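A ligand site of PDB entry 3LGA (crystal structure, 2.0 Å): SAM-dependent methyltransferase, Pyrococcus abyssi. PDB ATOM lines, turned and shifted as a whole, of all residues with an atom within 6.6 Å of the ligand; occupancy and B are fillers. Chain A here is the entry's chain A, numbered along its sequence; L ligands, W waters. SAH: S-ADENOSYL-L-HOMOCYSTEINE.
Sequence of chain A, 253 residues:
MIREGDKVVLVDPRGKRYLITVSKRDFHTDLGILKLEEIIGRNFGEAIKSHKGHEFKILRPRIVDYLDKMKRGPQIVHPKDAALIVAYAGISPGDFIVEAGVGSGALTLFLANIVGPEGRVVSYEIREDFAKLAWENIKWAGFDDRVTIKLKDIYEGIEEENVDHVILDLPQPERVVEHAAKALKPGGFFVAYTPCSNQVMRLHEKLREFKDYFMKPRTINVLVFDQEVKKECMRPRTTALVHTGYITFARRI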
ATOM      1  N   MET A  70      16.877 -10.224 -24.622  1.00  0.00           N
ATOM      2  CA  MET A  70      16.365 -11.524 -24.185  1.00  0.00           C
ATOM      3  C   MET A  70      17.371 -12.627 -24.571  1.00  0.00           C
ATOM      4  O   MET A  70      18.007 -12.555 -25.623  1.00  0.00           O
ATOM      5  CB  MET A  70      15.142 -11.766 -25.043  1.00  0.00           C
ATOM      6  CG  MET A  70      13.936 -12.352 -24.479  1.00  0.00           C
ATOM      7  SD  MET A  70      13.048 -12.860 -26.015  1.00  0.00           S
ATOM      8  CE  MET A  70      12.956 -11.379 -26.920  1.00  0.00           C
ATOM      9  N   GLN A  75      14.808 -20.056 -33.160  1.00  0.00           N
ATOM     10  CA  GLN A  75      13.477 -19.807 -33.760  1.00  0.00           C
ATOM     11  C   GLN A  75      12.505 -19.003 -32.878  1.00  0.00           C
ATOM     12  O   GLN A  75      11.838 -19.552 -32.009  1.00  0.00           O
ATOM     13  CB  GLN A  75      12.800 -21.106 -34.225  1.00  0.00           C
ATOM     14  CG  GLN A  75      13.093 -21.495 -35.677  1.00  0.00           C
ATOM     15  CD  GLN A  75      14.238 -22.462 -35.804  1.00  0.00           C
ATOM     16  OE1 GLN A  75      14.409 -23.359 -34.960  1.00  0.00           O
ATOM     17  NE2 GLN A  75      15.062 -22.293 -36.853  1.00  0.00           N
ATOM     18  N   ILE A  76      12.417 -17.704 -33.153  1.00  0.00           N
ATOM     19  CA  ILE A  76      11.518 -16.810 -32.429  1.00  0.00           C
ATOM     20  C   ILE A  76      10.478 -16.198 -33.389  1.00  0.00           C
ATOM     21  O   ILE A  76      10.629 -16.243 -34.618  1.00  0.00           O
ATOM     22  CB  ILE A  76      12.307 -15.702 -31.680  1.00  0.00           C
ATOM     23  CG1 ILE A  76      13.216 -14.907 -32.642  1.00  0.00           C
ATOM     24  CG2 ILE A  76      13.168 -16.306 -30.530  1.00  0.00           C
ATOM     25  CD1 ILE A  76      13.214 -13.420 -32.437  1.00  0.00           C
ATOM     26  N   VAL A  77       9.388 -15.665 -32.837  1.00  0.00           N
ATOM     27  CA  VAL A  77       8.536 -14.818 -33.661  1.00  0.00           C
ATOM     28  C   VAL A  77       9.147 -13.396 -33.593  1.00  0.00           C
ATOM     29  O   VAL A  77       9.354 -12.871 -32.499  1.00  0.00           O
ATOM     30  CB  VAL A  77       7.076 -14.891 -33.232  1.00  0.00           C
ATOM     31  CG1 VAL A  77       6.247 -13.850 -33.934  1.00  0.00           C
ATOM     32  CG2 VAL A  77       6.533 -16.327 -33.498  1.00  0.00           C
ATOM     33  N   HIS A  78       9.449 -12.827 -34.764  1.00  0.00           N
ATOM     34  CA  HIS A  78       9.987 -11.448 -34.933  1.00  0.00           C
ATOM     35  C   HIS A  78       8.972 -10.424 -34.453  1.00  0.00           C
ATOM     36  O   HIS A  78       7.777 -10.614 -34.661  1.00  0.00           O
ATOM     37  CB  HIS A  78      10.310 -11.162 -36.423  1.00  0.00           C
ATOM     38  CG  HIS A  78      11.003  -9.846 -36.686  1.00  0.00           C
ATOM     39  ND1 HIS A  78      12.257  -9.759 -37.260  1.00  0.00           N
ATOM     40  CD2 HIS A  78      10.589  -8.571 -36.499  1.00  0.00           C
ATOM     41  CE1 HIS A  78      12.592  -8.492 -37.383  1.00  0.00           C
ATOM     42  NE2 HIS A  78      11.606  -7.752 -36.918  1.00  0.00           N
ATOM     43  N   GLU A  99      -1.331 -19.613 -25.658  1.00  0.00           N
ATOM     44  CA  GLU A  99      -0.276 -19.656 -26.666  1.00  0.00           C
ATOM     45  C   GLU A  99       0.516 -20.989 -26.638  1.00  0.00           C
ATOM     46  O   GLU A  99       0.580 -21.649 -25.598  1.00  0.00           O
ATOM     47  CB  GLU A  99       0.579 -18.378 -26.562  1.00  0.00           C
ATOM     48  CG  GLU A  99       1.880 -18.428 -25.925  1.00  0.00           C
ATOM     49  CD  GLU A  99       2.984 -18.424 -26.932  1.00  0.00           C
ATOM     50  OE1 GLU A  99       3.568 -17.346 -27.226  1.00  0.00           O
ATOM     51  OE2 GLU A  99       3.313 -19.517 -27.424  1.00  0.00           O
ATOM     52  N   ALA A 100       1.044 -21.409 -27.783  1.00  0.00           N
ATOM     53  CA  ALA A 100       1.914 -22.610 -27.841  1.00  0.00           C
ATOM     54  C   ALA A 100       2.708 -22.562 -29.153  1.00  0.00           C
ATOM     55  O   ALA A 100       2.133 -22.145 -30.159  1.00  0.00           O
ATOM     56  CB  ALA A 100       1.084 -23.885 -27.785  1.00  0.00           C
ATOM     57  N   GLY A 101       3.967 -22.996 -29.170  1.00  0.00           N
ATOM     58  CA  GLY A 101       4.745 -23.404 -27.970  1.00  0.00           C
ATOM     59  C   GLY A 101       5.408 -22.151 -27.428  1.00  0.00           C
ATOM     60  O   GLY A 101       5.574 -21.194 -28.165  1.00  0.00           O
ATOM     61  N   VAL A 102       5.801 -22.126 -26.164  1.00  0.00           N
ATOM     62  CA  VAL A 102       6.419 -20.932 -25.588  1.00  0.00           C
ATOM     63  C   VAL A 102       7.771 -20.595 -26.256  1.00  0.00           C
ATOM     64  O   VAL A 102       8.112 -19.424 -26.385  1.00  0.00           O
ATOM     65  CB  VAL A 102       6.508 -20.993 -24.016  1.00  0.00           C
ATOM     66  CG1 VAL A 102       7.718 -21.805 -23.558  1.00  0.00           C
ATOM     67  CG2 VAL A 102       6.553 -19.558 -23.398  1.00  0.00           C
ATOM     68  N   GLY A 103       8.561 -21.595 -26.641  1.00  0.00           N
ATOM     69  CA  GLY A 103       9.850 -21.311 -27.282  1.00  0.00           C
ATOM     70  C   GLY A 103      10.828 -20.598 -26.344  1.00  0.00           C
ATOM     71  O   GLY A 103      11.008 -20.990 -25.188  1.00  0.00           O
ATOM     72  N   SER A 104      11.434 -19.530 -26.832  1.00  0.00           N
ATOM     73  CA  SER A 104      12.271 -18.688 -25.997  1.00  0.00           C
ATOM     74  C   SER A 104      11.474 -17.638 -25.234  1.00  0.00           C
ATOM     75  O   SER A 104      12.003 -16.948 -24.375  1.00  0.00           O
ATOM     76  CB  SER A 104      13.317 -17.959 -26.877  1.00  0.00           C
ATOM     77  OG  SER A 104      14.001 -18.889 -27.709  1.00  0.00           O
ATOM     78  N   GLY A 105      10.189 -17.516 -25.529  1.00  0.00           N
ATOM     79  CA  GLY A 105       9.390 -16.507 -24.794  1.00  0.00           C
ATOM     80  C   GLY A 105       9.255 -15.167 -25.491  1.00  0.00           C
ATOM     81  O   GLY A 105       8.708 -14.254 -24.916  1.00  0.00           O
ATOM     82  N   ALA A 106       9.756 -15.042 -26.720  1.00  0.00           N
ATOM     83  CA  ALA A 106       9.738 -13.719 -27.413  1.00  0.00           C
ATOM     84  C   ALA A 106       8.325 -13.218 -27.733  1.00  0.00           C
ATOM     85  O   ALA A 106       7.955 -12.093 -27.390  1.00  0.00           O
ATOM     86  CB  ALA A 106      10.612 -13.760 -28.716  1.00  0.00           C
ATOM     87  N   LEU A 107       7.523 -14.068 -28.361  1.00  0.00           N
ATOM     88  CA  LEU A 107       6.138 -13.744 -28.614  1.00  0.00           C
ATOM     89  C   LEU A 107       5.432 -13.579 -27.265  1.00  0.00           C
ATOM     90  O   LEU A 107       4.658 -12.649 -27.026  1.00  0.00           O
ATOM     91  CB  LEU A 107       5.505 -14.853 -29.466  1.00  0.00           C
ATOM     92  CG  LEU A 107       4.037 -14.596 -29.762  1.00  0.00           C
ATOM     93  CD1 LEU A 107       3.746 -13.214 -30.351  1.00  0.00           C
ATOM     94  CD2 LEU A 107       3.481 -15.699 -30.629  1.00  0.00           C
ATOM     95  N   THR A 108       5.707 -14.499 -26.336  1.00  0.00           N
ATOM     96  CA  THR A 108       5.065 -14.376 -25.011  1.00  0.00           C
ATOM     97  C   THR A 108       5.324 -13.031 -24.300  1.00  0.00           C
ATOM     98  O   THR A 108       4.378 -12.451 -23.787  1.00  0.00           O
ATOM     99  CB  THR A 108       5.540 -15.520 -24.083  1.00  0.00           C
ATOM    100  OG1 THR A 108       5.449 -16.731 -24.824  1.00  0.00           O
ATOM    101  CG2 THR A 108       4.636 -15.617 -22.816  1.00  0.00           C
ATOM    102  N   TYR A 124       1.687 -23.163 -23.499  1.00  0.00           N
ATOM    103  CA  TYR A 124       2.016 -24.597 -23.470  1.00  0.00           C
ATOM    104  C   TYR A 124       3.351 -24.854 -24.150  1.00  0.00           C
ATOM    105  O   TYR A 124       3.736 -24.140 -25.083  1.00  0.00           O
ATOM    106  CB  TYR A 124       0.926 -25.396 -24.181  1.00  0.00           C
ATOM    107  CG  TYR A 124      -0.423 -25.429 -23.499  1.00  0.00           C
ATOM    108  CD1 TYR A 124      -0.986 -26.639 -23.115  1.00  0.00           C
ATOM    109  CD2 TYR A 124      -1.185 -24.282 -23.339  1.00  0.00           C
ATOM    110  CE1 TYR A 124      -2.234 -26.696 -22.532  1.00  0.00           C
ATOM    111  CE2 TYR A 124      -2.448 -24.313 -22.754  1.00  0.00           C
ATOM    112  CZ  TYR A 124      -2.967 -25.527 -22.343  1.00  0.00           C
ATOM    113  OH  TYR A 124      -4.203 -25.577 -21.756  1.00  0.00           O
ATOM    114  N   GLU A 125       4.103 -25.809 -23.629  1.00  0.00           N
ATOM    115  CA  GLU A 125       5.396 -26.145 -24.162  1.00  0.00           C
ATOM    116  C   GLU A 125       5.678 -27.634 -23.875  1.00  0.00           C
ATOM    117  O   GLU A 125       5.307 -28.151 -22.823  1.00  0.00           O
ATOM    118  CB  GLU A 125       6.508 -25.281 -23.507  1.00  0.00           C
ATOM    119  CG  GLU A 125       7.950 -25.591 -23.945  1.00  0.00           C
ATOM    120  CD  GLU A 125       8.151 -25.561 -25.478  1.00  0.00           C
ATOM    121  OE1 GLU A 125       8.494 -26.628 -26.033  1.00  0.00           O
ATOM    122  OE2 GLU A 125       7.987 -24.495 -26.127  1.00  0.00           O
ATOM    123  N   ILE A 126       6.345 -28.317 -24.801  1.00  0.00           N
ATOM    124  CA  ILE A 126       6.690 -29.744 -24.617  1.00  0.00           C
ATOM    125  C   ILE A 126       8.175 -29.995 -24.357  1.00  0.00           C
ATOM    126  O   ILE A 126       8.533 -31.096 -23.900  1.00  0.00           O
ATOM    127  CB  ILE A 126       6.218 -30.646 -25.802  1.00  0.00           C
ATOM    128  CG1 ILE A 126       6.896 -30.244 -27.132  1.00  0.00           C
ATOM    129  CG2 ILE A 126       4.717 -30.661 -25.902  1.00  0.00           C
ATOM    130  CD1 ILE A 126       6.415 -31.091 -28.306  1.00  0.00           C
ATOM    131  N   ARG A 127       9.027 -29.005 -24.603  1.00  0.00           N
ATOM    132  CA  ARG A 127      10.449 -29.162 -24.283  1.00  0.00           C
ATOM    133  C   ARG A 127      10.815 -28.422 -22.997  1.00  0.00           C
ATOM    134  O   ARG A 127      10.722 -27.202 -22.972  1.00  0.00           O
ATOM    135  CB  ARG A 127      11.320 -28.652 -25.425  1.00  0.00           C
ATOM    136  CG  ARG A 127      11.245 -29.538 -26.679  1.00  0.00           C
ATOM    137  CD  ARG A 127      12.224 -29.083 -27.719  1.00  0.00           C
ATOM    138  NE  ARG A 127      13.604 -29.108 -27.196  1.00  0.00           N
ATOM    139  CZ  ARG A 127      14.709 -29.080 -27.947  1.00  0.00           C
ATOM    140  NH1 ARG A 127      14.610 -29.055 -29.281  1.00  0.00           N
ATOM    141  NH2 ARG A 127      15.926 -29.082 -27.371  1.00  0.00           N
ATOM    142  N   PHE A 130      13.306 -25.462 -23.099  1.00  0.00           N
ATOM    143  CA  PHE A 130      12.713 -24.212 -23.611  1.00  0.00           C
ATOM    144  C   PHE A 130      11.757 -23.611 -22.599  1.00  0.00           C
ATOM    145  O   PHE A 130      11.716 -22.396 -22.457  1.00  0.00           O
ATOM    146  CB  PHE A 130      11.988 -24.391 -24.958  1.00  0.00           C
ATOM    147  CG  PHE A 130      12.865 -24.841 -26.097  1.00  0.00           C
ATOM    148  CD1 PHE A 130      12.295 -25.375 -27.251  1.00  0.00           C
ATOM    149  CD2 PHE A 130      14.247 -24.778 -26.027  1.00  0.00           C
ATOM    150  CE1 PHE A 130      13.087 -25.827 -28.324  1.00  0.00           C
ATOM    151  CE2 PHE A 130      15.063 -25.217 -27.092  1.00  0.00           C
ATOM    152  CZ  PHE A 130      14.490 -25.739 -28.228  1.00  0.00           C
ATOM    153  N   LYS A 150       2.879 -23.989 -18.973  1.00  0.00           N
ATOM    154  CA  LYS A 150       2.462 -25.376 -18.747  1.00  0.00           C
ATOM    155  C   LYS A 150       3.347 -26.329 -19.566  1.00  0.00           C
ATOM    156  O   LYS A 150       3.564 -26.122 -20.783  1.00  0.00           O
ATOM    157  CB  LYS A 150       1.009 -25.557 -19.172  1.00  0.00           C
ATOM    158  CG  LYS A 150       0.024 -24.844 -18.273  1.00  0.00           C
ATOM    159  CD  LYS A 150      -1.413 -25.095 -18.790  1.00  0.00           C
ATOM    160  CE  LYS A 150      -2.414 -24.522 -17.801  1.00  0.00           C
ATOM    161  NZ  LYS A 150      -3.765 -25.073 -18.105  1.00  0.00           N
ATOM    162  N   LYS A 152       3.034 -29.258 -21.201  1.00  0.00           N
ATOM    163  CA  LYS A 152       1.887 -30.003 -21.628  1.00  0.00           C
ATOM    164  C   LYS A 152       1.760 -29.844 -23.141  1.00  0.00           C
ATOM    165  O   LYS A 152       2.070 -28.785 -23.686  1.00  0.00           O
ATOM    166  CB  LYS A 152       0.597 -29.497 -20.944  1.00  0.00           C
ATOM    167  CG  LYS A 152      -0.498 -30.602 -20.990  1.00  0.00           C
ATOM    168  CD  LYS A 152      -1.646 -30.433 -19.958  1.00  0.00           C
ATOM    169  CE  LYS A 152      -2.382 -31.800 -19.769  1.00  0.00           C
ATOM    170  NZ  LYS A 152      -3.657 -31.708 -18.979  1.00  0.00           N
ATOM    171  N   ASP A 153       1.292 -30.889 -23.799  1.00  0.00           N
ATOM    172  CA  ASP A 153       1.166 -30.930 -25.252  1.00  0.00           C
ATOM    173  C   ASP A 153      -0.198 -30.393 -25.634  1.00  0.00           C
ATOM    174  O   ASP A 153      -1.224 -30.989 -25.293  1.00  0.00           O
ATOM    175  CB  ASP A 153       1.367 -32.371 -25.787  1.00  0.00           C
ATOM    176  CG  ASP A 153       1.417 -32.429 -27.323  1.00  0.00           C
ATOM    177  OD1 ASP A 153       2.174 -33.262 -27.850  1.00  0.00           O
ATOM    178  OD2 ASP A 153       0.729 -31.654 -28.000  1.00  0.00           O
ATOM    179  N   ILE A 154      -0.242 -29.251 -26.324  1.00  0.00           N
ATOM    180  CA  ILE A 154      -1.536 -28.610 -26.629  1.00  0.00           C
ATOM    181  C   ILE A 154      -2.368 -29.371 -27.657  1.00  0.00           C
ATOM    182  O   ILE A 154      -3.584 -29.163 -27.755  1.00  0.00           O
ATOM    183  CB  ILE A 154      -1.358 -27.106 -27.058  1.00  0.00           C
ATOM    184  CG1 ILE A 154      -2.669 -26.336 -26.849  1.00  0.00           C
ATOM    185  CG2 ILE A 154      -0.838 -27.000 -28.482  1.00  0.00           C
ATOM    186  CD1 ILE A 154      -2.558 -24.787 -27.083  1.00  0.00           C
ATOM    187  N   TYR A 155      -1.752 -30.288 -28.398  1.00  0.00           N
ATOM    188  CA  TYR A 155      -2.536 -31.159 -29.329  1.00  0.00           C
ATOM    189  C   TYR A 155      -3.504 -32.074 -28.588  1.00  0.00           C
ATOM    190  O   TYR A 155      -4.459 -32.589 -29.189  1.00  0.00           O
ATOM    191  CB  TYR A 155      -1.622 -32.048 -30.166  1.00  0.00           C
ATOM    192  CG  TYR A 155      -0.670 -31.341 -31.079  1.00  0.00           C
ATOM    193  CD1 TYR A 155       0.503 -31.952 -31.459  1.00  0.00           C
ATOM    194  CD2 TYR A 155      -0.938 -30.028 -31.564  1.00  0.00           C
ATOM    195  CE1 TYR A 155       1.411 -31.324 -32.302  1.00  0.00           C
ATOM    196  CE2 TYR A 155      -0.032 -29.400 -32.429  1.00  0.00           C
ATOM    197  CZ  TYR A 155       1.125 -30.037 -32.789  1.00  0.00           C
ATOM    198  OH  TYR A 155       2.086 -29.426 -33.610  1.00  0.00           O
ATOM    199  N   GLU A 156      -3.272 -32.248 -27.281  1.00  0.00           N
ATOM    200  CA  GLU A 156      -4.113 -33.120 -26.488  1.00  0.00           C
ATOM    201  C   GLU A 156      -5.298 -32.345 -25.930  1.00  0.00           C
ATOM    202  O   GLU A 156      -6.227 -32.950 -25.421  1.00  0.00           O
ATOM    203  CB  GLU A 156      -3.325 -33.731 -25.332  1.00  0.00           C
ATOM    204  CG  GLU A 156      -2.322 -34.802 -25.713  1.00  0.00           C
ATOM    205  CD  GLU A 156      -2.866 -35.764 -26.799  1.00  0.00           C
ATOM    206  OE1 GLU A 156      -2.251 -35.833 -27.883  1.00  0.00           O
ATOM    207  OE2 GLU A 156      -3.892 -36.445 -26.575  1.00  0.00           O
ATOM    208  N   LEU A 168      -0.717 -19.477 -32.048  1.00  0.00           N
ATOM    209  CA  LEU A 168       0.148 -20.679 -32.227  1.00  0.00           C
ATOM    210  C   LEU A 168       1.364 -20.447 -33.083  1.00  0.00           C
ATOM    211  O   LEU A 168       1.281 -19.770 -34.090  1.00  0.00           O
ATOM    212  CB  LEU A 168      -0.674 -21.797 -32.879  1.00  0.00           C
ATOM    213  CG  LEU A 168      -1.965 -22.142 -32.090  1.00  0.00           C
ATOM    214  CD1 LEU A 168      -2.806 -23.108 -32.931  1.00  0.00           C
ATOM    215  CD2 LEU A 168      -1.578 -22.819 -30.731  1.00  0.00           C
ATOM    216  N   ASP A 169       2.489 -20.978 -32.641  1.00  0.00           N
ATOM    217  CA  ASP A 169       3.712 -21.074 -33.417  1.00  0.00           C
ATOM    218  C   ASP A 169       4.192 -22.500 -33.095  1.00  0.00           C
ATOM    219  O   ASP A 169       4.995 -22.709 -32.150  1.00  0.00           O
ATOM    220  CB  ASP A 169       4.738 -20.036 -32.935  1.00  0.00           C
ATOM    221  CG  ASP A 169       6.093 -20.194 -33.642  1.00  0.00           C
ATOM    222  OD1 ASP A 169       6.219 -21.068 -34.531  1.00  0.00           O
ATOM    223  OD2 ASP A 169       7.042 -19.459 -33.289  1.00  0.00           O
ATOM    224  N   LEU A 170       3.644 -23.446 -33.862  1.00  0.00           N
ATOM    225  CA  LEU A 170       3.602 -24.913 -33.623  1.00  0.00           C
ATOM    226  C   LEU A 170       3.844 -25.537 -34.998  1.00  0.00           C
ATOM    227  O   LEU A 170       3.340 -24.963 -35.945  1.00  0.00           O
ATOM    228  CB  LEU A 170       2.080 -25.356 -33.220  1.00  0.00           C
ATOM    229  CG  LEU A 170       2.196 -25.280 -31.743  1.00  0.00           C
ATOM    230  CD1 LEU A 170       1.290 -26.119 -30.903  1.00  0.00           C
ATOM    231  CD2 LEU A 170       3.560 -25.864 -31.775  1.00  0.00           C
ATOM    232  N   PRO A 171       4.491 -26.740 -35.118  1.00  0.00           N
ATOM    233  CA  PRO A 171       4.527 -27.359 -36.485  1.00  0.00           C
ATOM    234  C   PRO A 171       3.189 -27.697 -37.115  1.00  0.00           C
ATOM    235  O   PRO A 171       3.061 -27.608 -38.360  1.00  0.00           O
ATOM    236  CB  PRO A 171       5.367 -28.652 -36.272  1.00  0.00           C
ATOM    237  CG  PRO A 171       6.233 -28.321 -35.119  1.00  0.00           C
ATOM    238  CD  PRO A 171       5.307 -27.511 -34.178  1.00  0.00           C
ATOM    239  N   GLN A 172       2.188 -28.042 -36.292  1.00  0.00           N
ATOM    240  CA  GLN A 172       0.897 -28.510 -36.811  1.00  0.00           C
ATOM    241  C   GLN A 172      -0.332 -27.836 -36.224  1.00  0.00           C
ATOM    242  O   GLN A 172      -1.174 -28.509 -35.598  1.00  0.00           O
ATOM    243  CB  GLN A 172       0.763 -30.042 -36.642  1.00  0.00           C
ATOM    244  CG  GLN A 172       1.871 -30.814 -37.314  1.00  0.00           C
ATOM    245  CD  GLN A 172       1.794 -32.343 -37.038  1.00  0.00           C
ATOM    246  OE1 GLN A 172       1.490 -33.118 -37.930  1.00  0.00           O
ATOM    247  NE2 GLN A 172       2.088 -32.739 -35.807  1.00  0.00           N
ATOM    248  N   VAL A 176      -4.847 -28.173 -33.601  1.00  0.00           N
ATOM    249  CA  VAL A 176      -5.381 -27.352 -32.481  1.00  0.00           C
ATOM    250  C   VAL A 176      -6.710 -26.679 -32.815  1.00  0.00           C
ATOM    251  O   VAL A 176      -7.334 -26.094 -31.933  1.00  0.00           O
ATOM    252  CB  VAL A 176      -4.341 -26.287 -31.987  1.00  0.00           C
ATOM    253  CG1 VAL A 176      -4.767 -25.656 -30.650  1.00  0.00           C
ATOM    254  CG2 VAL A 176      -2.993 -26.926 -31.780  1.00  0.00           C
ATOM    255  N   TYR A 193       1.110 -18.885 -36.720  1.00  0.00           N
ATOM    256  CA  TYR A 193       2.273 -18.487 -37.457  1.00  0.00           C
ATOM    257  C   TYR A 193       2.920 -19.749 -38.053  1.00  0.00           C
ATOM    258  O   TYR A 193       3.171 -20.705 -37.311  1.00  0.00           O
ATOM    259  CB  TYR A 193       3.221 -17.806 -36.471  1.00  0.00           C
ATOM    260  CG  TYR A 193       4.642 -17.542 -36.985  1.00  0.00           C
ATOM    261  CD1 TYR A 193       5.635 -18.518 -36.866  1.00  0.00           C
ATOM    262  CD2 TYR A 193       4.973 -16.311 -37.556  1.00  0.00           C
ATOM    263  CE1 TYR A 193       6.956 -18.273 -37.317  1.00  0.00           C
ATOM    264  CE2 TYR A 193       6.268 -16.057 -38.019  1.00  0.00           C
ATOM    265  CZ  TYR A 193       7.237 -17.036 -37.898  1.00  0.00           C
ATOM    266  OH  TYR A 193       8.478 -16.744 -38.311  1.00  0.00           O
HETATM  267  N   SAH L   1       6.884 -18.246 -30.637  1.00  0.00           N
HETATM  268  CA  SAH L   1       8.140 -18.563 -29.831  1.00  0.00           C
HETATM  269  CB  SAH L   1       8.929 -19.663 -30.558  1.00  0.00           C
HETATM  270  CG  SAH L   1       8.200 -21.015 -30.669  1.00  0.00           C
HETATM  271  SD  SAH L   1       9.245 -22.294 -31.469  1.00  0.00           S
HETATM  272  C   SAH L   1       9.025 -17.324 -29.559  1.00  0.00           C
HETATM  273  O   SAH L   1       8.768 -16.268 -30.156  1.00  0.00           O
HETATM  274  OXT SAH L   1      10.018 -17.313 -28.788  1.00  0.00           O
HETATM  275  C5' SAH L   1       8.018 -23.670 -31.463  1.00  0.00           C
HETATM  276  C4' SAH L   1       7.851 -24.239 -30.048  1.00  0.00           C
HETATM  277  O4' SAH L   1       6.669 -25.018 -29.934  1.00  0.00           O
HETATM  278  C3' SAH L   1       9.005 -25.159 -29.650  1.00  0.00           C
HETATM  279  O3' SAH L   1       9.459 -24.650 -28.428  1.00  0.00           O
HETATM  280  C2' SAH L   1       8.358 -26.523 -29.480  1.00  0.00           C
HETATM  281  O2' SAH L   1       8.968 -27.257 -28.451  1.00  0.00           O
HETATM  282  C1' SAH L   1       6.927 -26.144 -29.123  1.00  0.00           C
HETATM  283  N9  SAH L   1       5.907 -27.140 -29.479  1.00  0.00           N
HETATM  284  C8  SAH L   1       5.873 -27.934 -30.600  1.00  0.00           C
HETATM  285  N7  SAH L   1       4.734 -28.685 -30.539  1.00  0.00           N
HETATM  286  C5  SAH L   1       4.079 -28.393 -29.403  1.00  0.00           C
HETATM  287  C6  SAH L   1       2.886 -28.878 -28.849  1.00  0.00           C
HETATM  288  N6  SAH L   1       2.162 -29.818 -29.489  1.00  0.00           N
HETATM  289  N1  SAH L   1       2.439 -28.358 -27.655  1.00  0.00           N
HETATM  290  C2  SAH L   1       3.165 -27.388 -26.997  1.00  0.00           C
HETATM  291  N3  SAH L   1       4.369 -26.905 -27.526  1.00  0.00           N
HETATM  292  C4  SAH L   1       4.798 -27.409 -28.717  1.00  0.00           C
HETATM  293  O   HOH W   1       6.780 -17.228 -27.078  1.00  0.00           O
HETATM  294  O   HOH W   2       9.664 -29.651 -29.898  1.00  0.00           O
HETATM  295  O   HOH W   3       4.655 -18.941 -29.367  1.00  0.00           O
HETATM  296  O   HOH W   4       4.918 -31.235 -31.748  1.00  0.00           O
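Merely in contact with the ligand: Gln 75 (3.3 Å), Ile 76 (3.6 Å), Val 102 (3.6 Å), Gly 103 (3.6 Å), Tyr 124 (3.7 Å), Ile 126 (3.7 Å), Arg 127 (3.7 Å), Phe 130 (3.2 Å), Lys 152 (3.8 Å), Tyr 155 (3.3 Å), Leu 170 (3.3 Å) and Pro 171 (3.6 Å).
Along chain A the residues within 4 Å of the ligand span positions 75 to 171.
The nearest printed residue that does not touch the ligand is Ala 100 (4.2 Å).
The side-chain carboxylate (OE2) of Glu 125 is in hydrogen-bond range of the backbone NH (N) of Val 102 (3.2 Å).
The backbone carbonyl oxygen of Lys 150 lies within hydrogen-bond range of the backbone NH of Glu 125 (2.9 Å).
The backbone NH (N) of Gly 103 lies within hydrogen-bond range of the side-chain carboxylate (OE2) of Glu 125 (3.0 Å).
O of Glu 125 sits at hydrogen-bond distance from N of Lys 152, 3.0 Å away.
The backbone NH (N) of Gly 101 is in hydrogen-bond range of the backbone carbonyl oxygen (O) of Asp 169.
The backbone NH (N) of Tyr 124 lies within hydrogen-bond range of the backbone carbonyl oxygen (O) of Glu 99 (2.8 Å).
N of Asp 169 sits at hydrogen-bond distance from O of Ala 100, at 2.8 Å.
OD2 of Asp 153 lies within hydrogen-bond range of N of Tyr 155.
Water W3 lies within hydrogen-bond range of the side-chain carboxylate (OE2) of Glu 99 (2.4 Å), a nitrogen (N) of the ligand (2.7 Å) and the backbone carbonyl oxygen (O) of Gly 101 (2.7 Å).
Water W1 lies within hydrogen-bond range of the backbone carbonyl oxygen of Val 102, the side-chain hydroxyl of Thr 108, the side-chain carboxylate of Glu 99 and the backbone NH of Leu 107.
An oxygen (OXT) of the ligand lies within hydrogen-bond range of the backbone NH (N) of Gly 105.
N of Ser 104 sits at hydrogen-bond distance from OXT of the ligand, at 3.3 Å.
The side-chain carboxylate (OE1) of Glu 125 lies within hydrogen-bond range of an oxygen (O2') of the ligand, at 2.5 Å.
An oxygen (O) of the ligand sits at hydrogen-bond distance from the backbone NH (N) of Leu 107 (3.1 Å).
An oxygen (O4') of the ligand lies close to the backbone NH (N) of Gly 101, 3.5 Å away.
A nitrogen (N1) of the ligand lies within hydrogen-bond range of the backbone NH of Ile 154.
An oxygen (OXT) of the ligand is in hydrogen-bond range of the backbone NH (N) of Ala 106, 3.1 Å away.
OD2 of Asp 169 lies within salt-bridge range of N of the ligand (2.9 Å).
O of the ligand is in hydrogen-bond range of N of Val 77 (2.8 Å).
OD2 of Asp 153 is in hydrogen-bond range of N6 of the ligand (2.8 Å).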
